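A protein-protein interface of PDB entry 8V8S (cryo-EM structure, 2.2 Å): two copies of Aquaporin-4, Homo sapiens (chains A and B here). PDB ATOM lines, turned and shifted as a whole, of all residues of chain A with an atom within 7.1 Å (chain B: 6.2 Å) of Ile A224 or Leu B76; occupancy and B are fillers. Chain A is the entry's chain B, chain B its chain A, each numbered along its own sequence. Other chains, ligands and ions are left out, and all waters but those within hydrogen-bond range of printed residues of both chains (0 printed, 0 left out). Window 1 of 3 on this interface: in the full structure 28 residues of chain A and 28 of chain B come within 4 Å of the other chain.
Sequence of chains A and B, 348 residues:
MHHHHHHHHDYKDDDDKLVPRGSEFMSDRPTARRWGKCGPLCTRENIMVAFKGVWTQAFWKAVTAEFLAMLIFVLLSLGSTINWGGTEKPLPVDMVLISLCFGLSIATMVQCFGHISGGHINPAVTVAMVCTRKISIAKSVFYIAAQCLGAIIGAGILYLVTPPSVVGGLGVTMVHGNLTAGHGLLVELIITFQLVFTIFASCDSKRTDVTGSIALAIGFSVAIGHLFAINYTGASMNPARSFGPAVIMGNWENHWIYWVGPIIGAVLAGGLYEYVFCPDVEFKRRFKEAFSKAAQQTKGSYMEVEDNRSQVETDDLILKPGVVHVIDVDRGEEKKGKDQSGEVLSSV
Printed residues of chain A that touch a printed residue of chain B: Ile A190, Gln A194, Thr A198, Phe A220, Ile A224, Leu A227 and Phe A228.
Printed residues of chain B that touch a printed residue of chain A: Leu B75, Leu B76, Gly B79, Ser B80, Cys B101, Leu B104, Ser B105 and Thr B108.
Among the printed residues, 13 pairs touch across the chains.
Among the printed residues, no Asp or Glu carboxylate lies within 4 Å of a Lys or Arg side-chain nitrogen of the other chain.
Of chain B, only Leu B76, Leu B104, Ser B105 and Thr B108 come within 4 Å of Ile A224.
Leu B76 touches two residues of chain A.
Of the printed residues of chain B, Gln A194 touches Thr B108 (3.4 Å).
Of the printed residues of chain A, Ser B105 touches Ile A224.
Printed residues of chain A within 4 Å of Leu B75: Ile A190 and Phe A228.
Printed residues of chain B within 4 Å of Ile A190: Leu B75 (3.6 Å).
Val A222 touches none of the printed residues of chain B.
The nearest residue of chain A that does not touch Leu B76 is Gln A194 (4.2 Å).
O of Ser B77 sits at hydrogen-bond distance from OG of Ser B80 (2.9 Å).
The side-chain hydroxyl (OG) of Ser B80 lies close to the side-chain sulfur (SG) of Cys B101, 3.6 Å away.
The backbone carbonyl oxygen of Ser A221 is in hydrogen-bond range of the side-chain amide nitrogen of Gln A194 (2.4 Å).
O of Gln A194 is in hydrogen-bond range of OG1 of Thr A198, at 3.2 Å.
The backbone carbonyl oxygen (O) of Cys B101 lies within hydrogen-bond range of the side-chain hydroxyl (OG) of Ser B105, at 2.6 Å.
OG of Ser B77 is in hydrogen-bond range of OG of Ser B105.
No position is printed for both chains.
Of the 13 pairs that touch across the chains among the printed residues, none has its exchanged pair printed and touching as well.
Ile A190 touches Leu B75.
OE1 of Gln A194 touches CG2 of Thr B108, at 3.4 Å.
Thr B108 touches Thr A198.
Ile A224 touches Leu B76 (CD1 to CD2, 3.8 Å).
Ser B105 touches Ile A224.
Thr B108 touches Ile A224 (OG1 to CD1, 3.5 Å).
Leu A227 touches Ser B80.
CD1 of Leu A227 touches N of Cys B101, at 3.9 Å.
CD2 of Phe A228 touches CD1 of Leu B76, 3.8 Å away.
CD1 of Phe A228 touches CA of Gly B79 (3.6 Å).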
ATOM      1  N   SER A  99     -27.137   8.420  -2.684  1.00  0.00           N
ATOM      2  CA  SER A  99     -26.048   7.470  -2.891  1.00  0.00           C
ATOM      3  C   SER A  99     -24.783   7.902  -2.157  1.00  0.00           C
ATOM      4  O   SER A  99     -24.136   7.093  -1.483  1.00  0.00           O
ATOM      5  CB  SER A  99     -25.773   7.308  -4.386  1.00  0.00           C
ATOM      6  OG  SER A  99     -26.933   6.880  -5.075  1.00  0.00           O
ATOM      7  N   GLY A 103     -22.975   6.149   1.064  1.00  0.00           N
ATOM      8  CA  GLY A 103     -21.626   5.654   0.845  1.00  0.00           C
ATOM      9  C   GLY A 103     -20.589   6.347   1.710  1.00  0.00           C
ATOM     10  O   GLY A 103     -19.735   5.696   2.315  1.00  0.00           O
ATOM     11  N   VAL A 187     -31.653  -8.822  -6.696  1.00  0.00           N
ATOM     12  CA  VAL A 187     -30.985  -7.525  -6.758  1.00  0.00           C
ATOM     13  C   VAL A 187     -30.211  -7.261  -5.471  1.00  0.00           C
ATOM     14  O   VAL A 187     -29.052  -6.832  -5.499  1.00  0.00           O
ATOM     15  CB  VAL A 187     -32.007  -6.409  -7.042  1.00  0.00           C
ATOM     16  CG1 VAL A 187     -31.388  -5.043  -6.794  1.00  0.00           C
ATOM     17  CG2 VAL A 187     -32.524  -6.514  -8.467  1.00  0.00           C
ATOM     18  N   ILE A 190     -26.873  -9.434  -5.115  1.00  0.00           N
ATOM     19  CA  ILE A 190     -25.692  -9.070  -5.891  1.00  0.00           C
ATOM     20  C   ILE A 190     -25.025  -7.819  -5.326  1.00  0.00           C
ATOM     21  O   ILE A 190     -23.795  -7.750  -5.229  1.00  0.00           O
ATOM     22  CB  ILE A 190     -26.069  -8.907  -7.375  1.00  0.00           C
ATOM     23  CG1 ILE A 190     -26.490 -10.259  -7.954  1.00  0.00           C
ATOM     24  CG2 ILE A 190     -24.906  -8.330  -8.165  1.00  0.00           C
ATOM     25  CD1 ILE A 190     -26.996 -10.198  -9.372  1.00  0.00           C
ATOM     26  N   ILE A 191     -25.818  -6.814  -4.943  1.00  0.00           N
ATOM     27  CA  ILE A 191     -25.229  -5.571  -4.449  1.00  0.00           C
ATOM     28  C   ILE A 191     -24.507  -5.797  -3.126  1.00  0.00           C
ATOM     29  O   ILE A 191     -23.518  -5.116  -2.829  1.00  0.00           O
ATOM     30  CB  ILE A 191     -26.296  -4.467  -4.326  1.00  0.00           C
ATOM     31  CG1 ILE A 191     -27.416  -4.891  -3.375  1.00  0.00           C
ATOM     32  CG2 ILE A 191     -26.855  -4.109  -5.697  1.00  0.00           C
ATOM     33  CD1 ILE A 191     -28.511  -3.861  -3.230  1.00  0.00           C
ATOM     34  N   GLN A 194     -21.005  -7.625  -3.977  1.00  0.00           N
ATOM     35  CA  GLN A 194     -19.911  -6.742  -4.369  1.00  0.00           C
ATOM     36  C   GLN A 194     -19.398  -5.922  -3.190  1.00  0.00           C
ATOM     37  O   GLN A 194     -18.228  -5.522  -3.181  1.00  0.00           O
ATOM     38  CB  GLN A 194     -20.357  -5.836  -5.521  1.00  0.00           C
ATOM     39  CG  GLN A 194     -21.306  -4.710  -5.132  1.00  0.00           C
ATOM     40  CD  GLN A 194     -20.585  -3.419  -4.799  1.00  0.00           C
ATOM     41  OE1 GLN A 194     -19.426  -3.229  -5.162  1.00  0.00           O
ATOM     42  NE2 GLN A 194     -21.273  -2.520  -4.105  1.00  0.00           N
ATOM     43  N   THR A 198     -15.500  -6.430  -1.691  1.00  0.00           N
ATOM     44  CA  THR A 198     -14.618  -5.275  -1.560  1.00  0.00           C
ATOM     45  C   THR A 198     -14.005  -5.205  -0.168  1.00  0.00           C
ATOM     46  O   THR A 198     -12.803  -4.949  -0.024  1.00  0.00           O
ATOM     47  CB  THR A 198     -15.389  -3.991  -1.878  1.00  0.00           C
ATOM     48  OG1 THR A 198     -15.515  -3.848  -3.297  1.00  0.00           O
ATOM     49  CG2 THR A 198     -14.668  -2.771  -1.319  1.00  0.00           C
ATOM     50  N   GLY A 219     -16.702   2.703   1.110  1.00  0.00           N
ATOM     51  CA  GLY A 219     -17.809   3.630   0.940  1.00  0.00           C
ATOM     52  C   GLY A 219     -18.301   3.708  -0.492  1.00  0.00           C
ATOM     53  O   GLY A 219     -19.509   3.726  -0.742  1.00  0.00           O
ATOM     54  N   PHE A 220     -17.375   3.758  -1.453  1.00  0.00           N
ATOM     55  CA  PHE A 220     -17.773   3.826  -2.854  1.00  0.00           C
ATOM     56  C   PHE A 220     -18.451   2.540  -3.309  1.00  0.00           C
ATOM     57  O   PHE A 220     -19.294   2.573  -4.211  1.00  0.00           O
ATOM     58  CB  PHE A 220     -16.561   4.135  -3.729  1.00  0.00           C
ATOM     59  CG  PHE A 220     -16.077   5.553  -3.610  1.00  0.00           C
ATOM     60  CD1 PHE A 220     -16.971   6.583  -3.365  1.00  0.00           C
ATOM     61  CD2 PHE A 220     -14.733   5.856  -3.736  1.00  0.00           C
ATOM     62  CE1 PHE A 220     -16.532   7.887  -3.252  1.00  0.00           C
ATOM     63  CE2 PHE A 220     -14.289   7.159  -3.623  1.00  0.00           C
ATOM     64  CZ  PHE A 220     -15.189   8.176  -3.381  1.00  0.00           C
ATOM     65  N   SER A 221     -18.101   1.405  -2.700  1.00  0.00           N
ATOM     66  CA  SER A 221     -18.811   0.164  -2.986  1.00  0.00           C
ATOM     67  C   SER A 221     -20.274   0.262  -2.569  1.00  0.00           C
ATOM     68  O   SER A 221     -21.164  -0.231  -3.271  1.00  0.00           O
ATOM     69  CB  SER A 221     -18.123  -1.007  -2.285  1.00  0.00           C
ATOM     70  OG  SER A 221     -18.739  -2.238  -2.615  1.00  0.00           O
ATOM     71  N   VAL A 222     -20.540   0.887  -1.419  1.00  0.00           N
ATOM     72  CA  VAL A 222     -21.918   1.145  -1.009  1.00  0.00           C
ATOM     73  C   VAL A 222     -22.586   2.124  -1.967  1.00  0.00           C
ATOM     74  O   VAL A 222     -23.757   1.962  -2.326  1.00  0.00           O
ATOM     75  CB  VAL A 222     -21.956   1.659   0.443  1.00  0.00           C
ATOM     76  CG1 VAL A 222     -23.340   2.187   0.792  1.00  0.00           C
ATOM     77  CG2 VAL A 222     -21.541   0.565   1.410  1.00  0.00           C
ATOM     78  N   ALA A 223     -21.850   3.155  -2.396  1.00  0.00           N
ATOM     79  CA  ALA A 223     -22.438   4.199  -3.229  1.00  0.00           C
ATOM     80  C   ALA A 223     -22.922   3.650  -4.568  1.00  0.00           C
ATOM     81  O   ALA A 223     -24.005   4.017  -5.037  1.00  0.00           O
ATOM     82  CB  ALA A 223     -21.429   5.327  -3.444  1.00  0.00           C
ATOM     83  N   ILE A 224     -22.135   2.776  -5.200  1.00  0.00           N
ATOM     84  CA  ILE A 224     -22.551   2.223  -6.485  1.00  0.00           C
ATOM     85  C   ILE A 224     -23.710   1.251  -6.330  1.00  0.00           C
ATOM     86  O   ILE A 224     -24.475   1.050  -7.280  1.00  0.00           O
ATOM     87  CB  ILE A 224     -21.371   1.547  -7.209  1.00  0.00           C
ATOM     88  CG1 ILE A 224     -20.909   0.299  -6.456  1.00  0.00           C
ATOM     89  CG2 ILE A 224     -20.230   2.523  -7.377  1.00  0.00           C
ATOM     90  CD1 ILE A 224     -19.775  -0.427  -7.134  1.00  0.00           C
ATOM     91  N   GLY A 225     -23.862   0.633  -5.157  1.00  0.00           N
ATOM     92  CA  GLY A 225     -25.041  -0.176  -4.913  1.00  0.00           C
ATOM     93  C   GLY A 225     -26.305   0.660  -4.862  1.00  0.00           C
ATOM     94  O   GLY A 225     -27.368   0.225  -5.315  1.00  0.00           O
ATOM     95  N   HIS A 226     -26.208   1.873  -4.311  1.00  0.00           N
ATOM     96  CA  HIS A 226     -27.364   2.761  -4.269  1.00  0.00           C
ATOM     97  C   HIS A 226     -27.656   3.352  -5.642  1.00  0.00           C
ATOM     98  O   HIS A 226     -28.822   3.457  -6.042  1.00  0.00           O
ATOM     99  CB  HIS A 226     -27.137   3.870  -3.244  1.00  0.00           C
ATOM    100  CG  HIS A 226     -27.533   3.491  -1.852  1.00  0.00           C
ATOM    101  ND1 HIS A 226     -26.736   2.714  -1.038  1.00  0.00           N
ATOM    102  CD2 HIS A 226     -28.645   3.770  -1.133  1.00  0.00           C
ATOM    103  CE1 HIS A 226     -27.338   2.538   0.125  1.00  0.00           C
ATOM    104  NE2 HIS A 226     -28.497   3.168   0.094  1.00  0.00           N
ATOM    105  N   LEU A 227     -26.613   3.723  -6.387  1.00  0.00           N
ATOM    106  CA  LEU A 227     -26.811   4.285  -7.718  1.00  0.00           C
ATOM    107  C   LEU A 227     -27.492   3.301  -8.657  1.00  0.00           C
ATOM    108  O   LEU A 227     -28.009   3.711  -9.702  1.00  0.00           O
ATOM    109  CB  LEU A 227     -25.472   4.728  -8.307  1.00  0.00           C
ATOM    110  CG  LEU A 227     -24.861   6.003  -7.725  1.00  0.00           C
ATOM    111  CD1 LEU A 227     -23.374   6.069  -8.029  1.00  0.00           C
ATOM    112  CD2 LEU A 227     -25.574   7.241  -8.247  1.00  0.00           C
ATOM    113  N   PHE A 228     -27.501   2.015  -8.309  1.00  0.00           N
ATOM    114  CA  PHE A 228     -28.151   0.977  -9.096  1.00  0.00           C
ATOM    115  C   PHE A 228     -29.538   0.612  -8.573  1.00  0.00           C
ATOM    116  O   PHE A 228     -30.500   0.588  -9.344  1.00  0.00           O
ATOM    117  CB  PHE A 228     -27.261  -0.273  -9.129  1.00  0.00           C
ATOM    118  CG  PHE A 228     -27.919  -1.479  -9.742  1.00  0.00           C
ATOM    119  CD1 PHE A 228     -28.649  -1.375 -10.915  1.00  0.00           C
ATOM    120  CD2 PHE A 228     -27.812  -2.719  -9.136  1.00  0.00           C
ATOM    121  CE1 PHE A 228     -29.254  -2.484 -11.470  1.00  0.00           C
ATOM    122  CE2 PHE A 228     -28.414  -3.832  -9.688  1.00  0.00           C
ATOM    123  CZ  PHE A 228     -29.136  -3.715 -10.858  1.00  0.00           C
ATOM    124  N   ALA A 229     -29.666   0.340  -7.273  1.00  0.00           N
ATOM    125  CA  ALA A 229     -30.803  -0.410  -6.752  1.00  0.00           C
ATOM    126  C   ALA A 229     -31.729   0.407  -5.853  1.00  0.00           C
ATOM    127  O   ALA A 229     -32.485  -0.177  -5.071  1.00  0.00           O
ATOM    128  CB  ALA A 229     -30.308  -1.646  -6.001  1.00  0.00           C
ATOM    129  N   ALA A 235     -32.014  -0.508  -2.312  1.00  0.00           N
ATOM    130  CA  ALA A 235     -30.567  -0.651  -2.142  1.00  0.00           C
ATOM    131  C   ALA A 235     -30.194  -0.715  -0.659  1.00  0.00           C
ATOM    132  O   ALA A 235     -29.488   0.145  -0.126  1.00  0.00           O
ATOM    133  CB  ALA A 235     -29.816   0.477  -2.857  1.00  0.00           C
ATOM    134  N   MET A 237     -28.795  -3.639   1.318  1.00  0.00           N
ATOM    135  CA  MET A 237     -27.526  -4.352   1.551  1.00  0.00           C
ATOM    136  C   MET A 237     -27.085  -4.292   3.011  1.00  0.00           C
ATOM    137  O   MET A 237     -25.896  -4.430   3.315  1.00  0.00           O
ATOM    138  CB  MET A 237     -26.390  -3.869   0.631  1.00  0.00           C
ATOM    139  CG  MET A 237     -26.173  -2.370   0.496  1.00  0.00           C
ATOM    140  SD  MET A 237     -25.137  -1.931  -0.910  1.00  0.00           S
ATOM    141  CE  MET A 237     -25.982  -0.464  -1.483  1.00  0.00           C
ATOM    142  N   LEU B  71     -19.023  -8.789 -15.185  1.00  0.00           N
ATOM    143  CA  LEU B  71     -20.448  -9.000 -14.949  1.00  0.00           C
ATOM    144  C   LEU B  71     -20.999  -7.996 -13.943  1.00  0.00           C
ATOM    145  O   LEU B  71     -22.088  -7.445 -14.139  1.00  0.00           O
ATOM    146  CB  LEU B  71     -20.683 -10.436 -14.474  1.00  0.00           C
ATOM    147  CG  LEU B  71     -22.092 -11.006 -14.275  1.00  0.00           C
ATOM    148  CD1 LEU B  71     -22.029 -12.519 -14.336  1.00  0.00           C
ATOM    149  CD2 LEU B  71     -22.716 -10.576 -12.956  1.00  0.00           C
ATOM    150  N   ILE B  72     -20.265  -7.751 -12.857  1.00  0.00           N
ATOM    151  CA  ILE B  72     -20.727  -6.799 -11.854  1.00  0.00           C
ATOM    152  C   ILE B  72     -20.682  -5.379 -12.402  1.00  0.00           C
ATOM    153  O   ILE B  72     -21.594  -4.578 -12.164  1.00  0.00           O
ATOM    154  CB  ILE B  72     -19.896  -6.940 -10.564  1.00  0.00           C
ATOM    155  CG1 ILE B  72     -20.206  -8.272  -9.877  1.00  0.00           C
ATOM    156  CG2 ILE B  72     -20.167  -5.782  -9.618  1.00  0.00           C
ATOM    157  CD1 ILE B  72     -18.999  -8.928  -9.246  1.00  0.00           C
ATOM    158  N   PHE B  73     -19.628  -5.046 -13.150  1.00  0.00           N
ATOM    159  CA  PHE B  73     -19.500  -3.701 -13.704  1.00  0.00           C
ATOM    160  C   PHE B  73     -20.628  -3.392 -14.681  1.00  0.00           C
ATOM    161  O   PHE B  73     -21.189  -2.291 -14.665  1.00  0.00           O
ATOM    162  CB  PHE B  73     -18.139  -3.547 -14.381  1.00  0.00           C
ATOM    163  CG  PHE B  73     -18.027  -2.332 -15.259  1.00  0.00           C
ATOM    164  CD1 PHE B  73     -18.199  -1.062 -14.735  1.00  0.00           C
ATOM    165  CD2 PHE B  73     -17.738  -2.460 -16.608  1.00  0.00           C
ATOM    166  CE1 PHE B  73     -18.092   0.056 -15.541  1.00  0.00           C
ATOM    167  CE2 PHE B  73     -17.630  -1.346 -17.418  1.00  0.00           C
ATOM    168  CZ  PHE B  73     -17.808  -0.087 -16.883  1.00  0.00           C
ATOM    169  N   VAL B  74     -20.977  -4.353 -15.539  1.00  0.00           N
ATOM    170  CA  VAL B  74     -22.025  -4.119 -16.527  1.00  0.00           C
ATOM    171  C   VAL B  74     -23.388  -4.022 -15.853  1.00  0.00           C
ATOM    172  O   VAL B  74     -24.188  -3.134 -16.168  1.00  0.00           O
ATOM    173  CB  VAL B  74     -21.996  -5.220 -17.603  1.00  0.00           C
ATOM    174  CG1 VAL B  74     -23.291  -5.230 -18.395  1.00  0.00           C
ATOM    175  CG2 VAL B  74     -20.815  -5.008 -18.530  1.00  0.00           C
ATOM    176  N   LEU B  75     -23.673  -4.927 -14.914  1.00  0.00           N
ATOM    177  CA  LEU B  75     -24.985  -4.952 -14.275  1.00  0.00           C
ATOM    178  C   LEU B  75     -25.250  -3.669 -13.494  1.00  0.00           C
ATOM    179  O   LEU B  75     -26.333  -3.081 -13.594  1.00  0.00           O
ATOM    180  CB  LEU B  75     -25.093  -6.170 -13.358  1.00  0.00           C
ATOM    181  CG  LEU B  75     -26.331  -6.239 -12.463  1.00  0.00           C
ATOM    182  CD1 LEU B  75     -27.601  -6.307 -13.294  1.00  0.00           C
ATOM    183  CD2 LEU B  75     -26.236  -7.427 -11.528  1.00  0.00           C
ATOM    184  N   LEU B  76     -24.269  -3.219 -12.710  1.00  0.00           N
ATOM    185  CA  LEU B  76     -24.490  -2.053 -11.860  1.00  0.00           C
ATOM    186  C   LEU B  76     -24.501  -0.762 -12.669  1.00  0.00           C
ATOM    187  O   LEU B  76     -25.321   0.126 -12.415  1.00  0.00           O
ATOM    188  CB  LEU B  76     -23.425  -1.994 -10.764  1.00  0.00           C
ATOM    189  CG  LEU B  76     -23.787  -2.608  -9.408  1.00  0.00           C
ATOM    190  CD1 LEU B  76     -24.274  -4.044  -9.556  1.00  0.00           C
ATOM    191  CD2 LEU B  76     -22.604  -2.538  -8.456  1.00  0.00           C
ATOM    192  N   SER B  77     -23.598  -0.639 -13.642  1.00  0.00           N
ATOM    193  CA  SER B  77     -23.499   0.601 -14.407  1.00  0.00           C
ATOM    194  C   SER B  77     -24.647   0.754 -15.399  1.00  0.00           C
ATOM    195  O   SER B  77     -25.211   1.846 -15.530  1.00  0.00           O
ATOM    196  CB  SER B  77     -22.156   0.663 -15.130  1.00  0.00           C
ATOM    197  OG  SER B  77     -21.081   0.668 -14.207  1.00  0.00           O
ATOM    198  N   LEU B  78     -25.006  -0.320 -16.108  1.00  0.00           N
ATOM    199  CA  LEU B  78     -26.121  -0.234 -17.047  1.00  0.00           C
ATOM    200  C   LEU B  78     -27.452  -0.084 -16.325  1.00  0.00           C
ATOM    201  O   LEU B  78     -28.388   0.508 -16.872  1.00  0.00           O
ATOM    202  CB  LEU B  78     -26.152  -1.460 -17.960  1.00  0.00           C
ATOM    203  CG  LEU B  78     -25.032  -1.599 -18.993  1.00  0.00           C
ATOM    204  CD1 LEU B  78     -25.366  -2.697 -19.990  1.00  0.00           C
ATOM    205  CD2 LEU B  78     -24.784  -0.281 -19.705  1.00  0.00           C
ATOM    206  N   GLY B  79     -27.562  -0.620 -15.109  1.00  0.00           N
ATOM    207  CA  GLY B  79     -28.773  -0.418 -14.335  1.00  0.00           C
ATOM    208  C   GLY B  79     -28.993   1.030 -13.952  1.00  0.00           C
ATOM    209  O   GLY B  79     -30.136   1.487 -13.865  1.00  0.00           O
ATOM    210  N   SER B  80     -27.909   1.773 -13.719  1.00  0.00           N
ATOM    211  CA  SER B  80     -28.028   3.165 -13.303  1.00  0.00           C
ATOM    212  C   SER B  80     -28.509   4.074 -14.426  1.00  0.00           C
ATOM    213  O   SER B  80     -29.011   5.167 -14.145  1.00  0.00           O
ATOM    214  CB  SER B  80     -26.688   3.670 -12.770  1.00  0.00           C
ATOM    215  OG  SER B  80     -25.855   4.120 -13.824  1.00  0.00           O
ATOM    216  N   THR B  81     -28.369   3.656 -15.681  1.00  0.00           N
ATOM    217  CA  THR B  81     -28.818   4.455 -16.813  1.00  0.00           C
ATOM    218  C   THR B  81     -30.289   4.230 -17.147  1.00  0.00           C
ATOM    219  O   THR B  81     -30.808   4.876 -18.064  1.00  0.00           O
ATOM    220  CB  THR B  81     -27.947   4.165 -18.045  1.00  0.00           C
ATOM    221  OG1 THR B  81     -27.946   5.305 -18.912  1.00  0.00           O
ATOM    222  CG2 THR B  81     -28.464   2.957 -18.809  1.00  0.00           C
ATOM    223  N   LEU B 100     -20.632   8.798 -12.286  1.00  0.00           N
ATOM    224  CA  LEU B 100     -20.025   8.263 -11.073  1.00  0.00           C
ATOM    225  C   LEU B 100     -20.250   6.763 -10.949  1.00  0.00           C
ATOM    226  O   LEU B 100     -19.363   6.037 -10.484  1.00  0.00           O
ATOM    227  CB  LEU B 100     -20.560   8.992  -9.841  1.00  0.00           C
ATOM    228  CG  LEU B 100     -19.848  10.290  -9.455  1.00  0.00           C
ATOM    229  CD1 LEU B 100     -19.393  11.033 -10.700  1.00  0.00           C
ATOM    230  CD2 LEU B 100     -20.752  11.168  -8.604  1.00  0.00           C
ATOM    231  N   CYS B 101     -21.424   6.274 -11.355  1.00  0.00           N
ATOM    232  CA  CYS B 101     -21.682   4.838 -11.276  1.00  0.00           C
ATOM    233  C   CYS B 101     -20.701   4.058 -12.139  1.00  0.00           C
ATOM    234  O   CYS B 101     -20.137   3.050 -11.699  1.00  0.00           O
ATOM    235  CB  CYS B 101     -23.119   4.528 -11.689  1.00  0.00           C
ATOM    236  SG  CYS B 101     -23.577   2.799 -11.426  1.00  0.00           S
ATOM    237  N   LEU B 104     -16.955   4.758 -10.535  1.00  0.00           N
ATOM    238  CA  LEU B 104     -16.691   4.120  -9.250  1.00  0.00           C
ATOM    239  C   LEU B 104     -16.829   2.603  -9.330  1.00  0.00           C
ATOM    240  O   LEU B 104     -16.200   1.887  -8.542  1.00  0.00           O
ATOM    241  CB  LEU B 104     -17.615   4.692  -8.176  1.00  0.00           C
ATOM    242  CG  LEU B 104     -17.486   6.185  -7.868  1.00  0.00           C
ATOM    243  CD1 LEU B 104     -18.476   6.595  -6.790  1.00  0.00           C
ATOM    244  CD2 LEU B 104     -16.063   6.534  -7.456  1.00  0.00           C
ATOM    245  N   SER B 105     -17.641   2.094 -10.260  1.00  0.00           N
ATOM    246  CA  SER B 105     -17.700   0.649 -10.464  1.00  0.00           C
ATOM    247  C   SER B 105     -16.357   0.111 -10.939  1.00  0.00           C
ATOM    248  O   SER B 105     -15.915  -0.956 -10.501  1.00  0.00           O
ATOM    249  CB  SER B 105     -18.797   0.293 -11.466  1.00  0.00           C
ATOM    250  OG  SER B 105     -20.083   0.523 -10.922  1.00  0.00           O
ATOM    251  N   THR B 108     -14.112   0.132  -8.079  1.00  0.00           N
ATOM    252  CA  THR B 108     -14.452  -0.947  -7.159  1.00  0.00           C
ATOM    253  C   THR B 108     -13.923  -2.290  -7.648  1.00  0.00           C
ATOM    254  O   THR B 108     -13.404  -3.082  -6.853  1.00  0.00           O
ATOM    255  CB  THR B 108     -15.968  -1.008  -6.961  1.00  0.00           C
ATOM    256  OG1 THR B 108     -16.438   0.257  -6.481  1.00  0.00           O
ATOM    257  CG2 THR B 108     -16.335  -2.087  -5.957  1.00  0.00           C
ATOM    258  N   MET B 109     -14.035  -2.561  -8.951  1.00  0.00           N
ATOM    259  CA  MET B 109     -13.584  -3.845  -9.478  1.00  0.00           C
ATOM    260  C   MET B 109     -12.064  -3.941  -9.530  1.00  0.00           C
ATOM    261  O   MET B 109     -11.509  -5.030  -9.342  1.00  0.00           O
ATOM    262  CB  MET B 109     -14.185  -4.088 -10.863  1.00  0.00           C
ATOM    263  CG  MET B 109     -15.708  -4.151 -10.890  1.00  0.00           C
ATOM    264  SD  MET B 109     -16.396  -5.611 -10.076  1.00  0.00           S
ATOM    265  CE  MET B 109     -16.772  -4.980  -8.441  1.00  0.00           C
